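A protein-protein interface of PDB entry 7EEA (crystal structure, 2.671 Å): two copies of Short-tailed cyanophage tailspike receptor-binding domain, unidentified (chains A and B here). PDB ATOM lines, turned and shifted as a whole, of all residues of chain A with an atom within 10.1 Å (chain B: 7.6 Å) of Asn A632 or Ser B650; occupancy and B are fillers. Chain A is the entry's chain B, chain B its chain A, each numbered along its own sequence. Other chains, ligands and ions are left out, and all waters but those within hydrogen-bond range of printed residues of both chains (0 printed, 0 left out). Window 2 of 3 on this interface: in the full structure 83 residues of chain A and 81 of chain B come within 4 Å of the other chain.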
ATOM      1  N   THR A 628      -3.915 -24.367 -19.595  1.00  0.00           N
ATOM      2  CA  THR A 628      -3.788 -23.336 -20.614  1.00  0.00           C
ATOM      3  C   THR A 628      -4.845 -22.272 -20.363  1.00  0.00           C
ATOM      4  O   THR A 628      -5.962 -22.580 -19.940  1.00  0.00           O
ATOM      5  CB  THR A 628      -3.928 -23.898 -22.035  1.00  0.00           C
ATOM      6  OG1 THR A 628      -5.306 -24.156 -22.326  1.00  0.00           O
ATOM      7  CG2 THR A 628      -3.140 -25.179 -22.172  1.00  0.00           C
ATOM      8  N   GLY A 629      -4.481 -21.017 -20.617  1.00  0.00           N
ATOM      9  CA  GLY A 629      -5.321 -19.890 -20.290  1.00  0.00           C
ATOM     10  C   GLY A 629      -6.195 -19.441 -21.451  1.00  0.00           C
ATOM     11  O   GLY A 629      -6.205 -20.020 -22.535  1.00  0.00           O
ATOM     12  N   THR A 630      -6.935 -18.366 -21.194  1.00  0.00           N
ATOM     13  CA  THR A 630      -7.878 -17.813 -22.152  1.00  0.00           C
ATOM     14  C   THR A 630      -7.465 -16.441 -22.669  1.00  0.00           C
ATOM     15  O   THR A 630      -8.176 -15.869 -23.503  1.00  0.00           O
ATOM     16  CB  THR A 630      -9.275 -17.744 -21.518  1.00  0.00           C
ATOM     17  OG1 THR A 630     -10.270 -17.679 -22.548  1.00  0.00           O
ATOM     18  CG2 THR A 630      -9.401 -16.526 -20.605  1.00  0.00           C
ATOM     19  N   VAL A 631      -6.337 -15.903 -22.206  1.00  0.00           N
ATOM     20  CA  VAL A 631      -5.839 -14.600 -22.620  1.00  0.00           C
ATOM     21  C   VAL A 631      -4.349 -14.721 -22.927  1.00  0.00           C
ATOM     22  O   VAL A 631      -3.739 -15.773 -22.741  1.00  0.00           O
ATOM     23  CB  VAL A 631      -6.090 -13.511 -21.556  1.00  0.00           C
ATOM     24  CG1 VAL A 631      -7.581 -13.311 -21.328  1.00  0.00           C
ATOM     25  CG2 VAL A 631      -5.385 -13.874 -20.263  1.00  0.00           C
ATOM     26  N   ASN A 632      -3.763 -13.617 -23.395  1.00  0.00           N
ATOM     27  CA  ASN A 632      -2.339 -13.573 -23.739  1.00  0.00           C
ATOM     28  C   ASN A 632      -1.520 -13.317 -22.472  1.00  0.00           C
ATOM     29  O   ASN A 632      -0.989 -12.231 -22.230  1.00  0.00           O
ATOM     30  CB  ASN A 632      -2.081 -12.513 -24.802  1.00  0.00           C
ATOM     31  CG  ASN A 632      -0.625 -12.456 -25.230  1.00  0.00           C
ATOM     32  OD1 ASN A 632       0.167 -13.341 -24.906  1.00  0.00           O
ATOM     33  ND2 ASN A 632      -0.267 -11.410 -25.966  1.00  0.00           N
ATOM     34  N   GLU A 633      -1.432 -14.360 -21.648  1.00  0.00           N
ATOM     35  CA  GLU A 633      -0.615 -14.345 -20.444  1.00  0.00           C
ATOM     36  C   GLU A 633       0.032 -15.711 -20.272  1.00  0.00           C
ATOM     37  O   GLU A 633      -0.457 -16.722 -20.781  1.00  0.00           O
ATOM     38  CB  GLU A 633      -1.432 -14.001 -19.191  1.00  0.00           C
ATOM     39  CG  GLU A 633      -2.087 -12.634 -19.211  1.00  0.00           C
ATOM     40  CD  GLU A 633      -3.128 -12.488 -18.124  1.00  0.00           C
ATOM     41  OE1 GLU A 633      -3.209 -13.388 -17.261  1.00  0.00           O
ATOM     42  OE2 GLU A 633      -3.869 -11.483 -18.131  1.00  0.00           O
ATOM     43  N   THR A 634       1.144 -15.731 -19.543  1.00  0.00           N
ATOM     44  CA  THR A 634       1.850 -16.970 -19.247  1.00  0.00           C
ATOM     45  C   THR A 634       1.350 -17.520 -17.918  1.00  0.00           C
ATOM     46  O   THR A 634       1.532 -16.889 -16.870  1.00  0.00           O
ATOM     47  CB  THR A 634       3.360 -16.745 -19.201  1.00  0.00           C
ATOM     48  OG1 THR A 634       3.833 -16.386 -20.506  1.00  0.00           O
ATOM     49  CG2 THR A 634       4.069 -18.012 -18.741  1.00  0.00           C
ATOM     50  N   PHE A 635       0.720 -18.689 -17.962  1.00  0.00           N
ATOM     51  CA  PHE A 635       0.183 -19.342 -16.779  1.00  0.00           C
ATOM     52  C   PHE A 635       1.058 -20.531 -16.406  1.00  0.00           C
ATOM     53  O   PHE A 635       1.585 -21.224 -17.282  1.00  0.00           O
ATOM     54  CB  PHE A 635      -1.260 -19.791 -17.013  1.00  0.00           C
ATOM     55  CG  PHE A 635      -2.181 -18.670 -17.407  1.00  0.00           C
ATOM     56  CD1 PHE A 635      -2.775 -17.874 -16.441  1.00  0.00           C
ATOM     57  CD2 PHE A 635      -2.447 -18.408 -18.741  1.00  0.00           C
ATOM     58  CE1 PHE A 635      -3.621 -16.840 -16.797  1.00  0.00           C
ATOM     59  CE2 PHE A 635      -3.292 -17.372 -19.102  1.00  0.00           C
ATOM     60  CZ  PHE A 635      -3.879 -16.589 -18.129  1.00  0.00           C
ATOM     61  N   SER A 649      -0.236 -16.268 -12.776  1.00  0.00           N
ATOM     62  CA  SER A 649      -0.042 -15.734 -14.114  1.00  0.00           C
ATOM     63  C   SER A 649       1.124 -14.754 -14.127  1.00  0.00           C
ATOM     64  O   SER A 649       1.601 -14.299 -13.084  1.00  0.00           O
ATOM     65  CB  SER A 649      -1.319 -15.049 -14.618  1.00  0.00           C
ATOM     66  OG  SER A 649      -1.037 -14.150 -15.677  1.00  0.00           O
ATOM     67  N   SER A 650       1.586 -14.436 -15.339  1.00  0.00           N
ATOM     68  CA  SER A 650       2.599 -13.402 -15.502  1.00  0.00           C
ATOM     69  C   SER A 650       2.048 -12.014 -15.205  1.00  0.00           C
ATOM     70  O   SER A 650       2.824 -11.101 -14.902  1.00  0.00           O
ATOM     71  CB  SER A 650       3.168 -13.447 -16.919  1.00  0.00           C
ATOM     72  OG  SER A 650       2.126 -13.473 -17.879  1.00  0.00           O
ATOM     73  N   ASN A 651       0.732 -11.840 -15.284  1.00  0.00           N
ATOM     74  CA  ASN A 651       0.075 -10.580 -14.957  1.00  0.00           C
ATOM     75  C   ASN A 651      -0.372 -10.642 -13.500  1.00  0.00           C
ATOM     76  O   ASN A 651      -1.320 -11.357 -13.162  1.00  0.00           O
ATOM     77  CB  ASN A 651      -1.101 -10.339 -15.902  1.00  0.00           C
ATOM     78  CG  ASN A 651      -1.944  -9.138 -15.511  1.00  0.00           C
ATOM     79  OD1 ASN A 651      -1.550  -8.322 -14.677  1.00  0.00           O
ATOM     80  ND2 ASN A 651      -3.116  -9.023 -16.124  1.00  0.00           N
ATOM     81  N   ALA A 652       0.308  -9.886 -12.635  1.00  0.00           N
ATOM     82  CA  ALA A 652      -0.022  -9.883 -11.215  1.00  0.00           C
ATOM     83  C   ALA A 652      -1.420  -9.349 -10.934  1.00  0.00           C
ATOM     84  O   ALA A 652      -1.877  -9.433  -9.788  1.00  0.00           O
ATOM     85  CB  ALA A 652       1.012  -9.064 -10.442  1.00  0.00           C
ATOM     86  N   SER A 654      -4.012 -10.514 -12.890  1.00  0.00           N
ATOM     87  CA  SER A 654      -4.782 -11.395 -13.756  1.00  0.00           C
ATOM     88  C   SER A 654      -6.153 -11.691 -13.166  1.00  0.00           C
ATOM     89  O   SER A 654      -6.300 -11.917 -11.961  1.00  0.00           O
ATOM     90  CB  SER A 654      -4.034 -12.706 -13.991  1.00  0.00           C
ATOM     91  OG  SER A 654      -3.260 -12.640 -15.172  1.00  0.00           O
ATOM     92  N   ALA A 656      -8.205 -13.738 -15.433  1.00  0.00           N
ATOM     93  CA  ALA A 656      -8.621 -14.592 -16.528  1.00  0.00           C
ATOM     94  C   ALA A 656      -9.086 -15.952 -16.021  1.00  0.00           C
ATOM     95  O   ALA A 656      -8.922 -16.309 -14.850  1.00  0.00           O
ATOM     96  CB  ALA A 656      -7.480 -14.774 -17.527  1.00  0.00           C
ATOM     97  N   THR A 657      -9.675 -16.716 -16.933  1.00  0.00           N
ATOM     98  CA  THR A 657     -10.052 -18.096 -16.682  1.00  0.00           C
ATOM     99  C   THR A 657      -9.011 -19.023 -17.295  1.00  0.00           C
ATOM    100  O   THR A 657      -8.522 -18.779 -18.403  1.00  0.00           O
ATOM    101  CB  THR A 657     -11.435 -18.408 -17.259  1.00  0.00           C
ATOM    102  OG1 THR A 657     -11.336 -18.580 -18.676  1.00  0.00           O
ATOM    103  CG2 THR A 657     -12.402 -17.274 -16.968  1.00  0.00           C
ATOM    104  N   VAL A 658      -8.666 -20.076 -16.564  1.00  0.00           N
ATOM    105  CA  VAL A 658      -7.728 -21.081 -17.043  1.00  0.00           C
ATOM    106  C   VAL A 658      -8.392 -22.446 -16.956  1.00  0.00           C
ATOM    107  O   VAL A 658      -9.219 -22.706 -16.075  1.00  0.00           O
ATOM    108  CB  VAL A 658      -6.401 -21.065 -16.253  1.00  0.00           C
ATOM    109  CG1 VAL A 658      -5.754 -19.692 -16.333  1.00  0.00           C
ATOM    110  CG2 VAL A 658      -6.632 -21.466 -14.805  1.00  0.00           C
ATOM    111  N   LEU B 603      -1.365 -22.620 -37.195  1.00  0.00           N
ATOM    112  CA  LEU B 603      -1.981 -21.303 -37.157  1.00  0.00           C
ATOM    113  C   LEU B 603      -1.758 -20.545 -38.464  1.00  0.00           C
ATOM    114  O   LEU B 603      -0.867 -20.854 -39.260  1.00  0.00           O
ATOM    115  CB  LEU B 603      -1.436 -20.488 -35.982  1.00  0.00           C
ATOM    116  CG  LEU B 603      -2.122 -20.686 -34.629  1.00  0.00           C
ATOM    117  CD1 LEU B 603      -1.765 -22.034 -34.028  1.00  0.00           C
ATOM    118  CD2 LEU B 603      -1.753 -19.570 -33.669  1.00  0.00           C
ATOM    119  N   GLY B 606      -1.954 -15.801 -36.885  1.00  0.00           N
ATOM    120  CA  GLY B 606      -2.016 -15.878 -35.443  1.00  0.00           C
ATOM    121  C   GLY B 606      -3.181 -16.650 -34.863  1.00  0.00           C
ATOM    122  O   GLY B 606      -3.317 -16.687 -33.635  1.00  0.00           O
ATOM    123  N   ASN B 632       8.428 -20.482 -29.606  1.00  0.00           N
ATOM    124  CA  ASN B 632       8.467 -19.581 -28.452  1.00  0.00           C
ATOM    125  C   ASN B 632       7.390 -18.504 -28.598  1.00  0.00           C
ATOM    126  O   ASN B 632       7.651 -17.338 -28.904  1.00  0.00           O
ATOM    127  CB  ASN B 632       9.853 -18.970 -28.303  1.00  0.00           C
ATOM    128  CG  ASN B 632       9.938 -17.985 -27.147  1.00  0.00           C
ATOM    129  OD1 ASN B 632       9.190 -18.086 -26.175  1.00  0.00           O
ATOM    130  ND2 ASN B 632      10.846 -17.024 -27.253  1.00  0.00           N
ATOM    131  N   GLU B 633       6.148 -18.921 -28.373  1.00  0.00           N
ATOM    132  CA  GLU B 633       5.009 -18.016 -28.362  1.00  0.00           C
ATOM    133  C   GLU B 633       4.050 -18.451 -27.265  1.00  0.00           C
ATOM    134  O   GLU B 633       4.012 -19.623 -26.885  1.00  0.00           O
ATOM    135  CB  GLU B 633       4.273 -17.995 -29.710  1.00  0.00           C
ATOM    136  CG  GLU B 633       5.155 -17.748 -30.923  1.00  0.00           C
ATOM    137  CD  GLU B 633       4.405 -17.919 -32.227  1.00  0.00           C
ATOM    138  OE1 GLU B 633       3.170 -18.105 -32.184  1.00  0.00           O
ATOM    139  OE2 GLU B 633       5.046 -17.869 -33.299  1.00  0.00           O
ATOM    140  N   THR B 634       3.281 -17.496 -26.753  1.00  0.00           N
ATOM    141  CA  THR B 634       2.205 -17.801 -25.822  1.00  0.00           C
ATOM    142  C   THR B 634       0.956 -18.158 -26.619  1.00  0.00           C
ATOM    143  O   THR B 634       0.529 -17.392 -27.490  1.00  0.00           O
ATOM    144  CB  THR B 634       1.927 -16.620 -24.891  1.00  0.00           C
ATOM    145  OG1 THR B 634       3.161 -16.128 -24.356  1.00  0.00           O
ATOM    146  CG2 THR B 634       1.014 -17.037 -23.748  1.00  0.00           C
ATOM    147  N   PHE B 635       0.389 -19.328 -26.334  1.00  0.00           N
ATOM    148  CA  PHE B 635      -0.787 -19.827 -27.035  1.00  0.00           C
ATOM    149  C   PHE B 635      -1.933 -19.971 -26.047  1.00  0.00           C
ATOM    150  O   PHE B 635      -1.754 -20.530 -24.959  1.00  0.00           O
ATOM    151  CB  PHE B 635      -0.497 -21.167 -27.714  1.00  0.00           C
ATOM    152  CG  PHE B 635       0.556 -21.089 -28.782  1.00  0.00           C
ATOM    153  CD1 PHE B 635       0.220 -20.736 -30.078  1.00  0.00           C
ATOM    154  CD2 PHE B 635       1.879 -21.371 -28.491  1.00  0.00           C
ATOM    155  CE1 PHE B 635       1.184 -20.666 -31.066  1.00  0.00           C
ATOM    156  CE2 PHE B 635       2.849 -21.301 -29.475  1.00  0.00           C
ATOM    157  CZ  PHE B 635       2.499 -20.949 -30.764  1.00  0.00           C
ATOM    158  N   TYR B 636      -3.107 -19.471 -26.426  1.00  0.00           N
ATOM    159  CA  TYR B 636      -4.266 -19.482 -25.548  1.00  0.00           C
ATOM    160  C   TYR B 636      -5.528 -19.703 -26.367  1.00  0.00           C
ATOM    161  O   TYR B 636      -5.555 -19.488 -27.581  1.00  0.00           O
ATOM    162  CB  TYR B 636      -4.378 -18.183 -24.735  1.00  0.00           C
ATOM    163  CG  TYR B 636      -4.357 -16.906 -25.551  1.00  0.00           C
ATOM    164  CD1 TYR B 636      -3.176 -16.433 -26.114  1.00  0.00           C
ATOM    165  CD2 TYR B 636      -5.514 -16.158 -25.734  1.00  0.00           C
ATOM    166  CE1 TYR B 636      -3.152 -15.265 -26.851  1.00  0.00           C
ATOM    167  CE2 TYR B 636      -5.497 -14.983 -26.465  1.00  0.00           C
ATOM    168  CZ  TYR B 636      -4.313 -14.541 -27.020  1.00  0.00           C
ATOM    169  OH  TYR B 636      -4.291 -13.377 -27.755  1.00  0.00           O
ATOM    170  N   VAL B 637      -6.577 -20.142 -25.678  1.00  0.00           N
ATOM    171  CA  VAL B 637      -7.866 -20.446 -26.286  1.00  0.00           C
ATOM    172  C   VAL B 637      -8.791 -19.266 -26.023  1.00  0.00           C
ATOM    173  O   VAL B 637      -9.215 -19.035 -24.884  1.00  0.00           O
ATOM    174  CB  VAL B 637      -8.451 -21.752 -25.734  1.00  0.00           C
ATOM    175  CG1 VAL B 637      -9.694 -22.155 -26.514  1.00  0.00           C
ATOM    176  CG2 VAL B 637      -7.406 -22.855 -25.774  1.00  0.00           C
ATOM    177  N   THR B 648      -5.436 -18.784 -30.507  1.00  0.00           N
ATOM    178  CA  THR B 648      -4.693 -17.621 -30.967  1.00  0.00           C
ATOM    179  C   THR B 648      -3.344 -17.551 -30.262  1.00  0.00           C
ATOM    180  O   THR B 648      -3.122 -18.196 -29.235  1.00  0.00           O
ATOM    181  CB  THR B 648      -5.473 -16.323 -30.732  1.00  0.00           C
ATOM    182  OG1 THR B 648      -5.269 -15.885 -29.387  1.00  0.00           O
ATOM    183  CG2 THR B 648      -6.957 -16.538 -30.959  1.00  0.00           C
ATOM    184  N   SER B 649      -2.443 -16.753 -30.830  1.00  0.00           N
ATOM    185  CA  SER B 649      -1.089 -16.619 -30.315  1.00  0.00           C
ATOM    186  C   SER B 649      -0.752 -15.151 -30.101  1.00  0.00           C
ATOM    187  O   SER B 649      -1.424 -14.254 -30.617  1.00  0.00           O
ATOM    188  CB  SER B 649      -0.060 -17.250 -31.263  1.00  0.00           C
ATOM    189  OG  SER B 649       1.250 -16.797 -30.963  1.00  0.00           O
ATOM    190  N   SER B 650       0.309 -14.919 -29.324  1.00  0.00           N
ATOM    191  CA  SER B 650       0.807 -13.561 -29.131  1.00  0.00           C
ATOM    192  C   SER B 650       1.276 -12.967 -30.450  1.00  0.00           C
ATOM    193  O   SER B 650       0.928 -11.832 -30.795  1.00  0.00           O
ATOM    194  CB  SER B 650       1.945 -13.558 -28.114  1.00  0.00           C
ATOM    195  OG  SER B 650       1.708 -14.501 -27.092  1.00  0.00           O
ATOM    196  N   ASN B 651       2.075 -13.723 -31.197  1.00  0.00           N
ATOM    197  CA  ASN B 651       2.545 -13.288 -32.507  1.00  0.00           C
ATOM    198  C   ASN B 651       1.359 -13.197 -33.457  1.00  0.00           C
ATOM    199  O   ASN B 651       0.823 -14.221 -33.894  1.00  0.00           O
ATOM    200  CB  ASN B 651       3.603 -14.258 -33.026  1.00  0.00           C
ATOM    201  CG  ASN B 651       4.023 -13.964 -34.454  1.00  0.00           C
ATOM    202  OD1 ASN B 651       3.851 -12.852 -34.951  1.00  0.00           O
ATOM    203  ND2 ASN B 651       4.580 -14.968 -35.120  1.00  0.00           N
ATOM    204  N   ALA B 652       0.945 -11.970 -33.781  1.00  0.00           N
ATOM    205  CA  ALA B 652      -0.182 -11.767 -34.686  1.00  0.00           C
ATOM    206  C   ALA B 652       0.094 -12.280 -36.094  1.00  0.00           C
ATOM    207  O   ALA B 652      -0.830 -12.317 -36.914  1.00  0.00           O
ATOM    208  CB  ALA B 652      -0.555 -10.285 -34.733  1.00  0.00           C
ATOM    209  N   ALA B 653       1.333 -12.667 -36.395  1.00  0.00           N
ATOM    210  CA  ALA B 653       1.683 -13.308 -37.655  1.00  0.00           C
ATOM    211  C   ALA B 653       2.104 -14.760 -37.445  1.00  0.00           C
ATOM    212  O   ALA B 653       2.988 -15.266 -38.143  1.00  0.00           O
ATOM    213  CB  ALA B 653       2.787 -12.528 -38.365  1.00  0.00           C
ATOM    214  N   SER B 654       1.482 -15.438 -36.483  1.00  0.00           N
ATOM    215  CA  SER B 654       1.865 -16.805 -36.157  1.00  0.00           C
ATOM    216  C   SER B 654       1.477 -17.766 -37.272  1.00  0.00           C
ATOM    217  O   SER B 654       0.408 -17.651 -37.878  1.00  0.00           O
ATOM    218  CB  SER B 654       1.213 -17.252 -34.850  1.00  0.00           C
ATOM    219  OG  SER B 654       2.050 -16.989 -33.742  1.00  0.00           O
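Ser B650 touches one residue of chain A. No residue of chain A comes within 4 Å of Ser B649. Printed residues of chain B within 4 Å of Val A631: Tyr B636 (3.1 Å). Of the printed residues of chain A, Tyr B636 touches Gly A629 (3.4 Å), Thr A630 (3.5 Å), Val A631 (3.1 Å) and Asn A632 (3.6 Å). The nearest printed residue of chain B that does not touch Thr A634 is Glu B633 (7.1 Å).
Asn A632 touches Thr B634, but with the chains exchanged Thr A634 does not touch Asn B632 (8.0 Å). Asn A632 touches Ser B650, but with the chains exchanged Ser A650 does not touch Asn B632 (11.8 Å). Glu A633 touches Thr B634, but with the chains exchanged Thr A634 does not touch Glu B633 (7.1 Å). Thr B634 touches its own counterpart, Thr A634. Positions printed for both chains: 632, 633, 634, 635, 649, 650, 651, 652 and 654. Of the 10 pairs that touch across the chains among the printed residues, 1 has its exchanged pair printed and touching as well.
Of the 15 printed residues of chain B, 4 touch a printed residue of chain A. Hydrophobic or aromatic side chains of chain B that line the printed part of chain A: Tyr B636. Of the 16 printed residues of chain A, 6 touch a printed residue of chain B. Among the printed residues, no Asp or Glu carboxylate lies within 4 Å of a Lys or Arg side-chain nitrogen of the other chain.
O of Gly A629 touches CB of Tyr B636 (3.4 Å). CD2 of Tyr B636 touches O of Thr A630 (3.5 Å). Tyr B636 touches Val A631. Asn A632 touches Thr B634. Tyr B636 touches Asn A632 (CE1 to CB, 3.6 Å). Glu A633 touches Thr B634. OG1 of Thr B634 touches OG1 of Thr A634, 3.9 Å away.
The backbone carbonyl oxygen of Thr B634 is in hydrogen-bond range of the backbone NH of Ser B650 (3.1 Å). The backbone NH (N) of Thr B648 lies within hydrogen-bond range of the backbone carbonyl oxygen (O) of Tyr B636 (3.0 Å). N of Thr A630 sits at hydrogen-bond distance from O of Thr A657 (3.2 Å). OE1 of Glu A633 lies within hydrogen-bond range of OG of Ser A649. The side-chain amide nitrogen of Asn A651 sits at hydrogen-bond distance from the side-chain carboxylate of Glu A633 (3.3 Å). The backbone carbonyl oxygen (O) of Thr A634 lies within hydrogen-bond range of the backbone NH (N) of Ser A650 (2.9 Å).
O of Gly A629 sits at hydrogen-bond distance from N of Val B637 (3.2 Å). The backbone carbonyl oxygen (O) of Val B637 lies within hydrogen-bond range of the side-chain hydroxyl (OG1) of Thr A630, 2.9 Å away. The side-chain hydroxyl of Ser B650 is in hydrogen-bond range of the side-chain amide oxygen of Asn A632, at 2.9 Å.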
